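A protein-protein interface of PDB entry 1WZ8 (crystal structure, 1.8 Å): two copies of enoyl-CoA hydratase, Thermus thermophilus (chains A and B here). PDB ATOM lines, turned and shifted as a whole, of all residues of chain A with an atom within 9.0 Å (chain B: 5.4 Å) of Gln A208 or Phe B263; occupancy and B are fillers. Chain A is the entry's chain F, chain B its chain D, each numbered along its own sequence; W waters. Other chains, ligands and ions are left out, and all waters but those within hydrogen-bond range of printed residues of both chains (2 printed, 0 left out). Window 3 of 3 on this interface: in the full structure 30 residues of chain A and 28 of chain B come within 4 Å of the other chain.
The chain-end carboxylate of Pro B264 is in salt-bridge range of the guanidinium group of Arg A56, 2.9 Å away. N of Lys A211 is in hydrogen-bond range of OE2 of Glu B247, at 3.2 Å. OE1 of Glu B247 lies within hydrogen-bond range of N of Ala A213 (3.1 Å). N of Glu A212 lies within hydrogen-bond range of OE2 of Glu B247 (2.7 Å).
The guanidinium group (NE) of Arg A56 lies within hydrogen-bond range of the backbone carbonyl oxygen (O) of Ala A207, 2.5 Å away. The backbone carbonyl oxygen (O) of Gly A209 is in hydrogen-bond range of the guanidinium group (NH2) of Arg A56, 2.8 Å away. The backbone carbonyl oxygen of Gly A20 is in hydrogen-bond range of the backbone NH of Arg A56 (2.9 Å).
Phe B263 touches Arg A56 (O to NH2, 3.99 Å). O of Gln A208 touches CD1 of Phe B263, at 3.5 Å. C of Gly A209 touches CD1 of Phe B263 (3.5 Å). Leu B142 touches Pro A210 (O to CG, 3.2 Å). Glu B247 touches Pro A210. N of Pro A210 touches CD1 of Phe B263 (3.4 Å). Leu B142 touches Ala A213 (CD1 to CB, 3.9 Å). Ala A213 touches Gly B145 (CB to O, 3.9 Å). Leu A214 touches Leu B142 (CD2 to CD1, 3.5 Å).
Gln A208 touches just one residue of chain B: Phe B263 (3.5 Å). Of the printed residues of chain A, Phe B263 touches Arg A56, Gln A208, Gly A209 and Pro A210. Pro B264 touches just one residue of chain A: Arg A56. Of the printed residues of chain B, Glu A212 touches Glu B247. Printed residues of chain A within 4 Å of Gly B145: Ala A213 (3.9 Å). Of the printed residues of chain B, Gly A209 touches Phe B263 (3.5 Å). Of the printed residues of chain B, Arg A56 touches Phe B263 (3.99 Å) and Pro B264 (2.9 Å). Of the printed residues of chain B, Pro A210 touches Leu B142, Glu B247 and Phe B263. Pro A19 touches none of the printed residues of chain B. The nearest printed residue of chain A that does not touch Phe B263 is Lys A211 (5.1 Å).
Hydrophobic or aromatic side chains of chain B within 4 Å of the printed part of chain A: Leu B142 and Phe B263. Of the 22 printed residues of chain A, 8 touch a printed residue of chain B.
No position is printed for both chains. Of the 13 pairs that touch across the chains among the printed residues, none has its exchanged pair printed and touching as well.
Water W2 lies within hydrogen-bond range of the chain-end carboxylate (O) of Pro B264 (2.5 Å), the side-chain carboxylate (OE2) of Glu B247 (2.9 Å), the backbone NH (N) of Lys A211 (3.0 Å) and the guanidinium group (NH2) of Arg A56 (3.1 Å). Water W1 lies within hydrogen-bond range of the backbone carbonyl oxygen (O) of Gln A208, the backbone carbonyl oxygen (O) of Pro B261 and the backbone NH (N) of Phe B263.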
ATOM      1  N   ARG A  18     -19.333 -23.489 -31.338  1.00  0.00           N
ATOM      2  CA  ARG A  18     -19.559 -24.613 -30.440  1.00  0.00           C
ATOM      3  C   ARG A  18     -20.146 -24.064 -29.143  1.00  0.00           C
ATOM      4  O   ARG A  18     -20.017 -22.875 -28.846  1.00  0.00           O
ATOM      5  CB  ARG A  18     -18.240 -25.341 -30.156  1.00  0.00           C
ATOM      6  CG  ARG A  18     -17.671 -26.110 -31.348  1.00  0.00           C
ATOM      7  CD  ARG A  18     -18.556 -27.298 -31.706  1.00  0.00           C
ATOM      8  NE  ARG A  18     -17.926 -28.195 -32.673  1.00  0.00           N
ATOM      9  CZ  ARG A  18     -17.768 -27.928 -33.966  1.00  0.00           C
ATOM     10  NH1 ARG A  18     -18.198 -26.779 -34.474  1.00  0.00           N
ATOM     11  NH2 ARG A  18     -17.177 -28.815 -34.755  1.00  0.00           N
ATOM     12  N   PRO A  19     -20.816 -24.920 -28.360  1.00  0.00           N
ATOM     13  CA  PRO A  19     -21.415 -24.483 -27.096  1.00  0.00           C
ATOM     14  C   PRO A  19     -20.412 -23.838 -26.142  1.00  0.00           C
ATOM     15  O   PRO A  19     -19.388 -24.437 -25.807  1.00  0.00           O
ATOM     16  CB  PRO A  19     -22.001 -25.775 -26.534  1.00  0.00           C
ATOM     17  CG  PRO A  19     -22.407 -26.513 -27.781  1.00  0.00           C
ATOM     18  CD  PRO A  19     -21.197 -26.309 -28.670  1.00  0.00           C
ATOM     19  N   GLY A  20     -20.708 -22.612 -25.720  1.00  0.00           N
ATOM     20  CA  GLY A  20     -19.833 -21.915 -24.793  1.00  0.00           C
ATOM     21  C   GLY A  20     -18.579 -21.333 -25.408  1.00  0.00           C
ATOM     22  O   GLY A  20     -17.781 -20.699 -24.715  1.00  0.00           O
ATOM     23  N   VAL A  21     -18.394 -21.541 -26.707  1.00  0.00           N
ATOM     24  CA  VAL A  21     -17.218 -21.013 -27.389  1.00  0.00           C
ATOM     25  C   VAL A  21     -17.550 -19.759 -28.187  1.00  0.00           C
ATOM     26  O   VAL A  21     -18.222 -19.831 -29.218  1.00  0.00           O
ATOM     27  CB  VAL A  21     -16.603 -22.062 -28.347  1.00  0.00           C
ATOM     28  CG1 VAL A  21     -15.434 -21.451 -29.111  1.00  0.00           C
ATOM     29  CG2 VAL A  21     -16.143 -23.271 -27.555  1.00  0.00           C
ATOM     30  N   ARG A  56     -17.431 -19.479 -22.127  1.00  0.00           N
ATOM     31  CA  ARG A  56     -16.610 -20.387 -21.338  1.00  0.00           C
ATOM     32  C   ARG A  56     -15.220 -20.458 -21.967  1.00  0.00           C
ATOM     33  O   ARG A  56     -14.276 -20.952 -21.359  1.00  0.00           O
ATOM     34  CB  ARG A  56     -17.250 -21.777 -21.272  1.00  0.00           C
ATOM     35  CG  ARG A  56     -18.612 -21.785 -20.579  1.00  0.00           C
ATOM     36  CD  ARG A  56     -19.268 -23.164 -20.617  1.00  0.00           C
ATOM     37  NE  ARG A  56     -18.654 -24.107 -19.685  1.00  0.00           N
ATOM     38  CZ  ARG A  56     -18.966 -24.206 -18.395  1.00  0.00           C
ATOM     39  NH1 ARG A  56     -19.893 -23.418 -17.866  1.00  0.00           N
ATOM     40  NH2 ARG A  56     -18.350 -25.103 -17.633  1.00  0.00           N
ATOM     41  N   ALA A  57     -15.109 -19.958 -23.195  1.00  0.00           N
ATOM     42  CA  ALA A  57     -13.835 -19.929 -23.907  1.00  0.00           C
ATOM     43  C   ALA A  57     -13.943 -18.997 -25.106  1.00  0.00           C
ATOM     44  O   ALA A  57     -15.012 -18.856 -25.705  1.00  0.00           O
ATOM     45  CB  ALA A  57     -13.453 -21.329 -24.371  1.00  0.00           C
ATOM     46  N   PRO A 106     -10.569 -18.926 -20.704  1.00  0.00           N
ATOM     47  CA  PRO A 106      -9.437 -19.350 -21.530  1.00  0.00           C
ATOM     48  C   PRO A 106      -9.597 -18.786 -22.941  1.00  0.00           C
ATOM     49  O   PRO A 106     -10.710 -18.729 -23.467  1.00  0.00           O
ATOM     50  CB  PRO A 106      -9.552 -20.875 -21.526  1.00  0.00           C
ATOM     51  CG  PRO A 106     -10.234 -21.174 -20.235  1.00  0.00           C
ATOM     52  CD  PRO A 106     -11.286 -20.092 -20.159  1.00  0.00           C
ATOM     53  N   LEU A 200     -10.487 -25.093 -32.723  1.00  0.00           N
ATOM     54  CA  LEU A 200     -11.887 -25.183 -32.316  1.00  0.00           C
ATOM     55  C   LEU A 200     -12.076 -26.336 -31.338  1.00  0.00           C
ATOM     56  O   LEU A 200     -12.811 -26.216 -30.357  1.00  0.00           O
ATOM     57  CB  LEU A 200     -12.791 -25.389 -33.538  1.00  0.00           C
ATOM     58  CG  LEU A 200     -14.293 -25.445 -33.238  1.00  0.00           C
ATOM     59  CD1 LEU A 200     -14.733 -24.170 -32.516  1.00  0.00           C
ATOM     60  CD2 LEU A 200     -15.070 -25.614 -34.543  1.00  0.00           C
ATOM     61  N   GLU A 201     -11.409 -27.451 -31.612  1.00  0.00           N
ATOM     62  CA  GLU A 201     -11.491 -28.626 -30.754  1.00  0.00           C
ATOM     63  C   GLU A 201     -11.002 -28.278 -29.350  1.00  0.00           C
ATOM     64  O   GLU A 201     -11.629 -28.641 -28.347  1.00  0.00           O
ATOM     65  CB  GLU A 201     -10.638 -29.749 -31.338  1.00  0.00           C
ATOM     66  CG  GLU A 201     -10.528 -30.973 -30.461  1.00  0.00           C
ATOM     67  CD  GLU A 201      -9.640 -32.029 -31.078  1.00  0.00           C
ATOM     68  OE1 GLU A 201     -10.019 -32.584 -32.129  1.00  0.00           O
ATOM     69  OE2 GLU A 201      -8.555 -32.296 -30.518  1.00  0.00           O
ATOM     70  N   VAL A 202      -9.880 -27.572 -29.292  1.00  0.00           N
ATOM     71  CA  VAL A 202      -9.299 -27.159 -28.016  1.00  0.00           C
ATOM     72  C   VAL A 202     -10.252 -26.217 -27.280  1.00  0.00           C
ATOM     73  O   VAL A 202     -10.501 -26.374 -26.080  1.00  0.00           O
ATOM     74  CB  VAL A 202      -7.940 -26.462 -28.237  1.00  0.00           C
ATOM     75  CG1 VAL A 202      -7.422 -25.868 -26.927  1.00  0.00           C
ATOM     76  CG2 VAL A 202      -6.938 -27.468 -28.795  1.00  0.00           C
ATOM     77  N   ALA A 203     -10.795 -25.243 -28.002  1.00  0.00           N
ATOM     78  CA  ALA A 203     -11.720 -24.294 -27.399  1.00  0.00           C
ATOM     79  C   ALA A 203     -12.938 -25.018 -26.836  1.00  0.00           C
ATOM     80  O   ALA A 203     -13.391 -24.719 -25.734  1.00  0.00           O
ATOM     81  CB  ALA A 203     -12.156 -23.255 -28.431  1.00  0.00           C
ATOM     82  N   GLU A 204     -13.468 -25.977 -27.589  1.00  0.00           N
ATOM     83  CA  GLU A 204     -14.641 -26.709 -27.129  1.00  0.00           C
ATOM     84  C   GLU A 204     -14.316 -27.523 -25.877  1.00  0.00           C
ATOM     85  O   GLU A 204     -15.135 -27.608 -24.962  1.00  0.00           O
ATOM     86  CB  GLU A 204     -15.181 -27.629 -28.231  1.00  0.00           C
ATOM     87  CG  GLU A 204     -16.536 -28.245 -27.880  1.00  0.00           C
ATOM     88  CD  GLU A 204     -17.155 -29.031 -29.023  1.00  0.00           C
ATOM     89  OE1 GLU A 204     -18.343 -29.406 -28.908  1.00  0.00           O
ATOM     90  OE2 GLU A 204     -16.463 -29.279 -30.031  1.00  0.00           O
ATOM     91  N   ARG A 205     -13.126 -28.115 -25.835  1.00  0.00           N
ATOM     92  CA  ARG A 205     -12.708 -28.901 -24.676  1.00  0.00           C
ATOM     93  C   ARG A 205     -12.673 -28.007 -23.442  1.00  0.00           C
ATOM     94  O   ARG A 205     -13.148 -28.389 -22.371  1.00  0.00           O
ATOM     95  CB  ARG A 205     -11.320 -29.515 -24.897  1.00  0.00           C
ATOM     96  CG  ARG A 205     -11.296 -30.730 -25.808  1.00  0.00           C
ATOM     97  CD  ARG A 205      -9.895 -31.348 -25.863  1.00  0.00           C
ATOM     98  NE  ARG A 205      -9.398 -31.719 -24.538  1.00  0.00           N
ATOM     99  CZ  ARG A 205      -8.205 -32.264 -24.308  1.00  0.00           C
ATOM    100  NH1 ARG A 205      -7.374 -32.506 -25.313  1.00  0.00           N
ATOM    101  NH2 ARG A 205      -7.843 -32.573 -23.070  1.00  0.00           N
ATOM    102  N   LEU A 206     -12.111 -26.813 -23.598  1.00  0.00           N
ATOM    103  CA  LEU A 206     -12.030 -25.866 -22.492  1.00  0.00           C
ATOM    104  C   LEU A 206     -13.430 -25.445 -22.052  1.00  0.00           C
ATOM    105  O   LEU A 206     -13.690 -25.277 -20.862  1.00  0.00           O
ATOM    106  CB  LEU A 206     -11.220 -24.638 -22.909  1.00  0.00           C
ATOM    107  CG  LEU A 206      -9.724 -24.896 -23.129  1.00  0.00           C
ATOM    108  CD1 LEU A 206      -9.131 -23.781 -23.976  1.00  0.00           C
ATOM    109  CD2 LEU A 206      -9.016 -25.003 -21.779  1.00  0.00           C
ATOM    110  N   ALA A 207     -14.333 -25.280 -23.014  1.00  0.00           N
ATOM    111  CA  ALA A 207     -15.701 -24.879 -22.701  1.00  0.00           C
ATOM    112  C   ALA A 207     -16.428 -25.983 -21.926  1.00  0.00           C
ATOM    113  O   ALA A 207     -17.375 -25.709 -21.182  1.00  0.00           O
ATOM    114  CB  ALA A 207     -16.455 -24.543 -23.992  1.00  0.00           C
ATOM    115  N   GLN A 208     -15.978 -27.226 -22.101  1.00  0.00           N
ATOM    116  CA  GLN A 208     -16.577 -28.368 -21.413  1.00  0.00           C
ATOM    117  C   GLN A 208     -15.890 -28.587 -20.071  1.00  0.00           C
ATOM    118  O   GLN A 208     -16.245 -29.501 -19.324  1.00  0.00           O
ATOM    119  CB  GLN A 208     -16.434 -29.652 -22.239  1.00  0.00           C
ATOM    120  CG  GLN A 208     -16.998 -29.580 -23.641  1.00  0.00           C
ATOM    121  CD  GLN A 208     -16.785 -30.874 -24.410  1.00  0.00           C
ATOM    122  OE1 GLN A 208     -15.698 -31.455 -24.383  1.00  0.00           O
ATOM    123  NE2 GLN A 208     -17.823 -31.328 -25.108  1.00  0.00           N
ATOM    124  N   GLY A 209     -14.896 -27.758 -19.776  1.00  0.00           N
ATOM    125  CA  GLY A 209     -14.181 -27.892 -18.522  1.00  0.00           C
ATOM    126  C   GLY A 209     -14.844 -27.107 -17.409  1.00  0.00           C
ATOM    127  O   GLY A 209     -15.843 -26.417 -17.640  1.00  0.00           O
ATOM    128  N   PRO A 210     -14.321 -27.198 -16.178  1.00  0.00           N
ATOM    129  CA  PRO A 210     -14.877 -26.479 -15.025  1.00  0.00           C
ATOM    130  C   PRO A 210     -14.540 -24.984 -15.062  1.00  0.00           C
ATOM    131  O   PRO A 210     -13.386 -24.587 -14.919  1.00  0.00           O
ATOM    132  CB  PRO A 210     -14.250 -27.203 -13.838  1.00  0.00           C
ATOM    133  CG  PRO A 210     -12.910 -27.586 -14.362  1.00  0.00           C
ATOM    134  CD  PRO A 210     -13.224 -28.090 -15.762  1.00  0.00           C
ATOM    135  N   LYS A 211     -15.570 -24.167 -15.246  1.00  0.00           N
ATOM    136  CA  LYS A 211     -15.455 -22.716 -15.354  1.00  0.00           C
ATOM    137  C   LYS A 211     -14.662 -22.005 -14.249  1.00  0.00           C
ATOM    138  O   LYS A 211     -13.695 -21.295 -14.530  1.00  0.00           O
ATOM    139  CB  LYS A 211     -16.865 -22.121 -15.444  1.00  0.00           C
ATOM    140  CG  LYS A 211     -16.949 -20.685 -15.917  1.00  0.00           C
ATOM    141  CD  LYS A 211     -18.412 -20.305 -16.166  1.00  0.00           C
ATOM    142  CE  LYS A 211     -18.546 -18.925 -16.792  1.00  0.00           C
ATOM    143  NZ  LYS A 211     -19.968 -18.590 -17.131  1.00  0.00           N
ATOM    144  N   GLU A 212     -15.080 -22.178 -13.001  1.00  0.00           N
ATOM    145  CA  GLU A 212     -14.393 -21.528 -11.888  1.00  0.00           C
ATOM    146  C   GLU A 212     -12.945 -21.986 -11.768  1.00  0.00           C
ATOM    147  O   GLU A 212     -12.038 -21.166 -11.610  1.00  0.00           O
ATOM    148  CB  GLU A 212     -15.106 -21.814 -10.565  1.00  0.00           C
ATOM    149  CG  GLU A 212     -14.372 -21.240  -9.361  1.00  0.00           C
ATOM    150  CD  GLU A 212     -15.076 -21.523  -8.048  1.00  0.00           C
ATOM    151  OE1 GLU A 212     -16.226 -21.073  -7.885  1.00  0.00           O
ATOM    152  OE2 GLU A 212     -14.477 -22.192  -7.178  1.00  0.00           O
ATOM    153  N   ALA A 213     -12.736 -23.295 -11.835  1.00  0.00           N
ATOM    154  CA  ALA A 213     -11.391 -23.851 -11.717  1.00  0.00           C
ATOM    155  C   ALA A 213     -10.469 -23.352 -12.828  1.00  0.00           C
ATOM    156  O   ALA A 213      -9.305 -23.054 -12.577  1.00  0.00           O
ATOM    157  CB  ALA A 213     -11.450 -25.364 -11.720  1.00  0.00           C
ATOM    158  N   LEU A 214     -10.990 -23.275 -14.052  1.00  0.00           N
ATOM    159  CA  LEU A 214     -10.207 -22.797 -15.188  1.00  0.00           C
ATOM    160  C   LEU A 214      -9.848 -21.329 -15.002  1.00  0.00           C
ATOM    161  O   LEU A 214      -8.719 -20.920 -15.268  1.00  0.00           O
ATOM    162  CB  LEU A 214     -10.994 -22.988 -16.490  1.00  0.00           C
ATOM    163  CG  LEU A 214     -10.979 -24.422 -17.032  1.00  0.00           C
ATOM    164  CD1 LEU A 214     -12.086 -24.617 -18.057  1.00  0.00           C
ATOM    165  CD2 LEU A 214      -9.616 -24.704 -17.646  1.00  0.00           C
ATOM    166  N   LEU B 142      -8.053 -30.113 -12.897  1.00  0.00           N
ATOM    167  CA  LEU B 142      -9.158 -29.624 -13.713  1.00  0.00           C
ATOM    168  C   LEU B 142     -10.192 -30.700 -14.043  1.00  0.00           C
ATOM    169  O   LEU B 142     -11.371 -30.403 -14.232  1.00  0.00           O
ATOM    170  CB  LEU B 142      -8.609 -28.974 -14.988  1.00  0.00           C
ATOM    171  CG  LEU B 142      -8.134 -27.515 -14.844  1.00  0.00           C
ATOM    172  CD1 LEU B 142      -9.355 -26.604 -14.756  1.00  0.00           C
ATOM    173  CD2 LEU B 142      -7.240 -27.338 -13.600  1.00  0.00           C
ATOM    174  N   ARG B 143      -9.747 -31.951 -14.101  1.00  0.00           N
ATOM    175  CA  ARG B 143     -10.638 -33.070 -14.378  1.00  0.00           C
ATOM    176  C   ARG B 143     -11.452 -33.334 -13.112  1.00  0.00           C
ATOM    177  O   ARG B 143     -12.601 -33.792 -13.154  1.00  0.00           O
ATOM    178  CB  ARG B 143      -9.816 -34.306 -14.727  1.00  0.00           C
ATOM    179  CG  ARG B 143     -10.667 -35.497 -15.082  1.00  0.00           C
ATOM    180  CD  ARG B 143     -10.370 -36.019 -16.471  1.00  0.00           C
ATOM    181  NE  ARG B 143     -11.446 -35.645 -17.382  1.00  0.00           N
ATOM    182  CZ  ARG B 143     -12.577 -36.323 -17.564  1.00  0.00           C
ATOM    183  NH1 ARG B 143     -12.816 -37.458 -16.910  1.00  0.00           N
ATOM    184  NH2 ARG B 143     -13.492 -35.834 -18.389  1.00  0.00           N
ATOM    185  N   LEU B 144     -10.827 -33.028 -11.983  1.00  0.00           N
ATOM    186  CA  LEU B 144     -11.425 -33.212 -10.673  1.00  0.00           C
ATOM    187  C   LEU B 144     -12.414 -32.090 -10.373  1.00  0.00           C
ATOM    188  O   LEU B 144     -13.341 -32.262  -9.582  1.00  0.00           O
ATOM    189  CB  LEU B 144     -10.309 -33.244  -9.623  1.00  0.00           C
ATOM    190  CG  LEU B 144     -10.589 -33.707  -8.193  1.00  0.00           C
ATOM    191  CD1 LEU B 144     -11.218 -35.097  -8.197  1.00  0.00           C
ATOM    192  CD2 LEU B 144      -9.276 -33.719  -7.422  1.00  0.00           C
ATOM    193  N   GLY B 145     -12.214 -30.935 -11.000  1.00  0.00           N
ATOM    194  CA  GLY B 145     -13.119 -29.823 -10.778  1.00  0.00           C
ATOM    195  C   GLY B 145     -12.592 -28.710  -9.894  1.00  0.00           C
ATOM    196  O   GLY B 145     -13.369 -27.902  -9.390  1.00  0.00           O
ATOM    197  N   GLU B 247     -18.519 -27.509  -8.741  1.00  0.00           N
ATOM    198  CA  GLU B 247     -17.644 -28.163  -9.716  1.00  0.00           C
ATOM    199  C   GLU B 247     -16.909 -29.372  -9.136  1.00  0.00           C
ATOM    200  O   GLU B 247     -16.795 -30.405  -9.793  1.00  0.00           O
ATOM    201  CB  GLU B 247     -16.655 -27.147 -10.308  1.00  0.00           C
ATOM    202  CG  GLU B 247     -17.348 -26.068 -11.135  1.00  0.00           C
ATOM    203  CD  GLU B 247     -16.416 -24.972 -11.622  1.00  0.00           C
ATOM    204  OE1 GLU B 247     -15.214 -25.009 -11.296  1.00  0.00           O
ATOM    205  OE2 GLU B 247     -16.899 -24.068 -12.334  1.00  0.00           O
ATOM    206  N   GLU B 250     -19.405 -32.293  -8.812  1.00  0.00           N
ATOM    207  CA  GLU B 250     -19.620 -32.966 -10.089  1.00  0.00           C
ATOM    208  C   GLU B 250     -18.387 -33.744 -10.539  1.00  0.00           C
ATOM    209  O   GLU B 250     -18.495 -34.861 -11.060  1.00  0.00           O
ATOM    210  CB  GLU B 250     -20.000 -31.932 -11.156  1.00  0.00           C
ATOM    211  CG  GLU B 250     -20.054 -32.454 -12.594  1.00  0.00           C
ATOM    212  CD  GLU B 250     -21.048 -33.585 -12.788  1.00  0.00           C
ATOM    213  OE1 GLU B 250     -21.916 -33.781 -11.911  1.00  0.00           O
ATOM    214  OE2 GLU B 250     -20.963 -34.274 -13.828  1.00  0.00           O
ATOM    215  N   GLY B 251     -17.217 -33.144 -10.341  1.00  0.00           N
ATOM    216  CA  GLY B 251     -15.977 -33.796 -10.724  1.00  0.00           C
ATOM    217  C   GLY B 251     -15.794 -35.104  -9.979  1.00  0.00           C
ATOM    218  O   GLY B 251     -15.382 -36.107 -10.562  1.00  0.00           O
ATOM    219  N   PRO B 261     -17.574 -35.786 -16.828  1.00  0.00           N
ATOM    220  CA  PRO B 261     -18.168 -34.729 -16.006  1.00  0.00           C
ATOM    221  C   PRO B 261     -18.996 -33.729 -16.801  1.00  0.00           C
ATOM    222  O   PRO B 261     -18.671 -33.395 -17.944  1.00  0.00           O
ATOM    223  CB  PRO B 261     -16.952 -34.084 -15.349  1.00  0.00           C
ATOM    224  CG  PRO B 261     -15.907 -34.211 -16.418  1.00  0.00           C
ATOM    225  CD  PRO B 261     -16.111 -35.630 -16.909  1.00  0.00           C
ATOM    226  N   GLU B 262     -20.078 -33.264 -16.186  1.00  0.00           N
ATOM    227  CA  GLU B 262     -20.960 -32.285 -16.802  1.00  0.00           C
ATOM    228  C   GLU B 262     -20.926 -31.056 -15.907  1.00  0.00           C
ATOM    229  O   GLU B 262     -21.837 -30.830 -15.108  1.00  0.00           O
ATOM    230  CB  GLU B 262     -22.385 -32.826 -16.885  1.00  0.00           C
ATOM    231  CG  GLU B 262     -23.302 -31.992 -17.756  1.00  0.00           C
ATOM    232  CD  GLU B 262     -22.885 -32.005 -19.215  1.00  0.00           C
ATOM    233  OE1 GLU B 262     -22.726 -33.112 -19.775  1.00  0.00           O
ATOM    234  OE2 GLU B 262     -22.724 -30.910 -19.798  1.00  0.00           O
ATOM    235  N   PHE B 263     -19.863 -30.268 -16.041  1.00  0.00           N
ATOM    236  CA  PHE B 263     -19.691 -29.070 -15.230  1.00  0.00           C
ATOM    237  C   PHE B 263     -20.742 -27.999 -15.510  1.00  0.00           C
ATOM    238  O   PHE B 263     -21.138 -27.786 -16.655  1.00  0.00           O
ATOM    239  CB  PHE B 263     -18.280 -28.513 -15.433  1.00  0.00           C
ATOM    240  CG  PHE B 263     -17.194 -29.434 -14.941  1.00  0.00           C
ATOM    241  CD1 PHE B 263     -16.243 -29.940 -15.816  1.00  0.00           C
ATOM    242  CD2 PHE B 263     -17.131 -29.803 -13.597  1.00  0.00           C
ATOM    243  CE1 PHE B 263     -15.242 -30.801 -15.366  1.00  0.00           C
ATOM    244  CE2 PHE B 263     -16.134 -30.662 -13.137  1.00  0.00           C
ATOM    245  CZ  PHE B 263     -15.187 -31.163 -14.027  1.00  0.00           C
ATOM    246  N   PRO B 264     -21.210 -27.309 -14.452  1.00  0.00           N
ATOM    247  CA  PRO B 264     -22.227 -26.250 -14.542  1.00  0.00           C
ATOM    248  C   PRO B 264     -21.802 -24.976 -15.269  1.00  0.00           C
ATOM    249  O   PRO B 264     -20.588 -24.745 -15.410  1.00  0.00           O
ATOM    250  CB  PRO B 264     -22.578 -25.988 -13.078  1.00  0.00           C
ATOM    251  CG  PRO B 264     -21.284 -26.252 -12.377  1.00  0.00           C
ATOM    252  CD  PRO B 264     -20.803 -27.523 -13.051  1.00  0.00           C
ATOM    253  OXT PRO B 264     -22.704 -24.210 -15.675  1.00  0.00           O
HETATM  254  O   HOH W   1     -18.658 -30.664 -18.790  1.00  0.00           O
HETATM  255  O   HOH W   2     -18.298 -25.327 -14.560  1.00  0.00           O
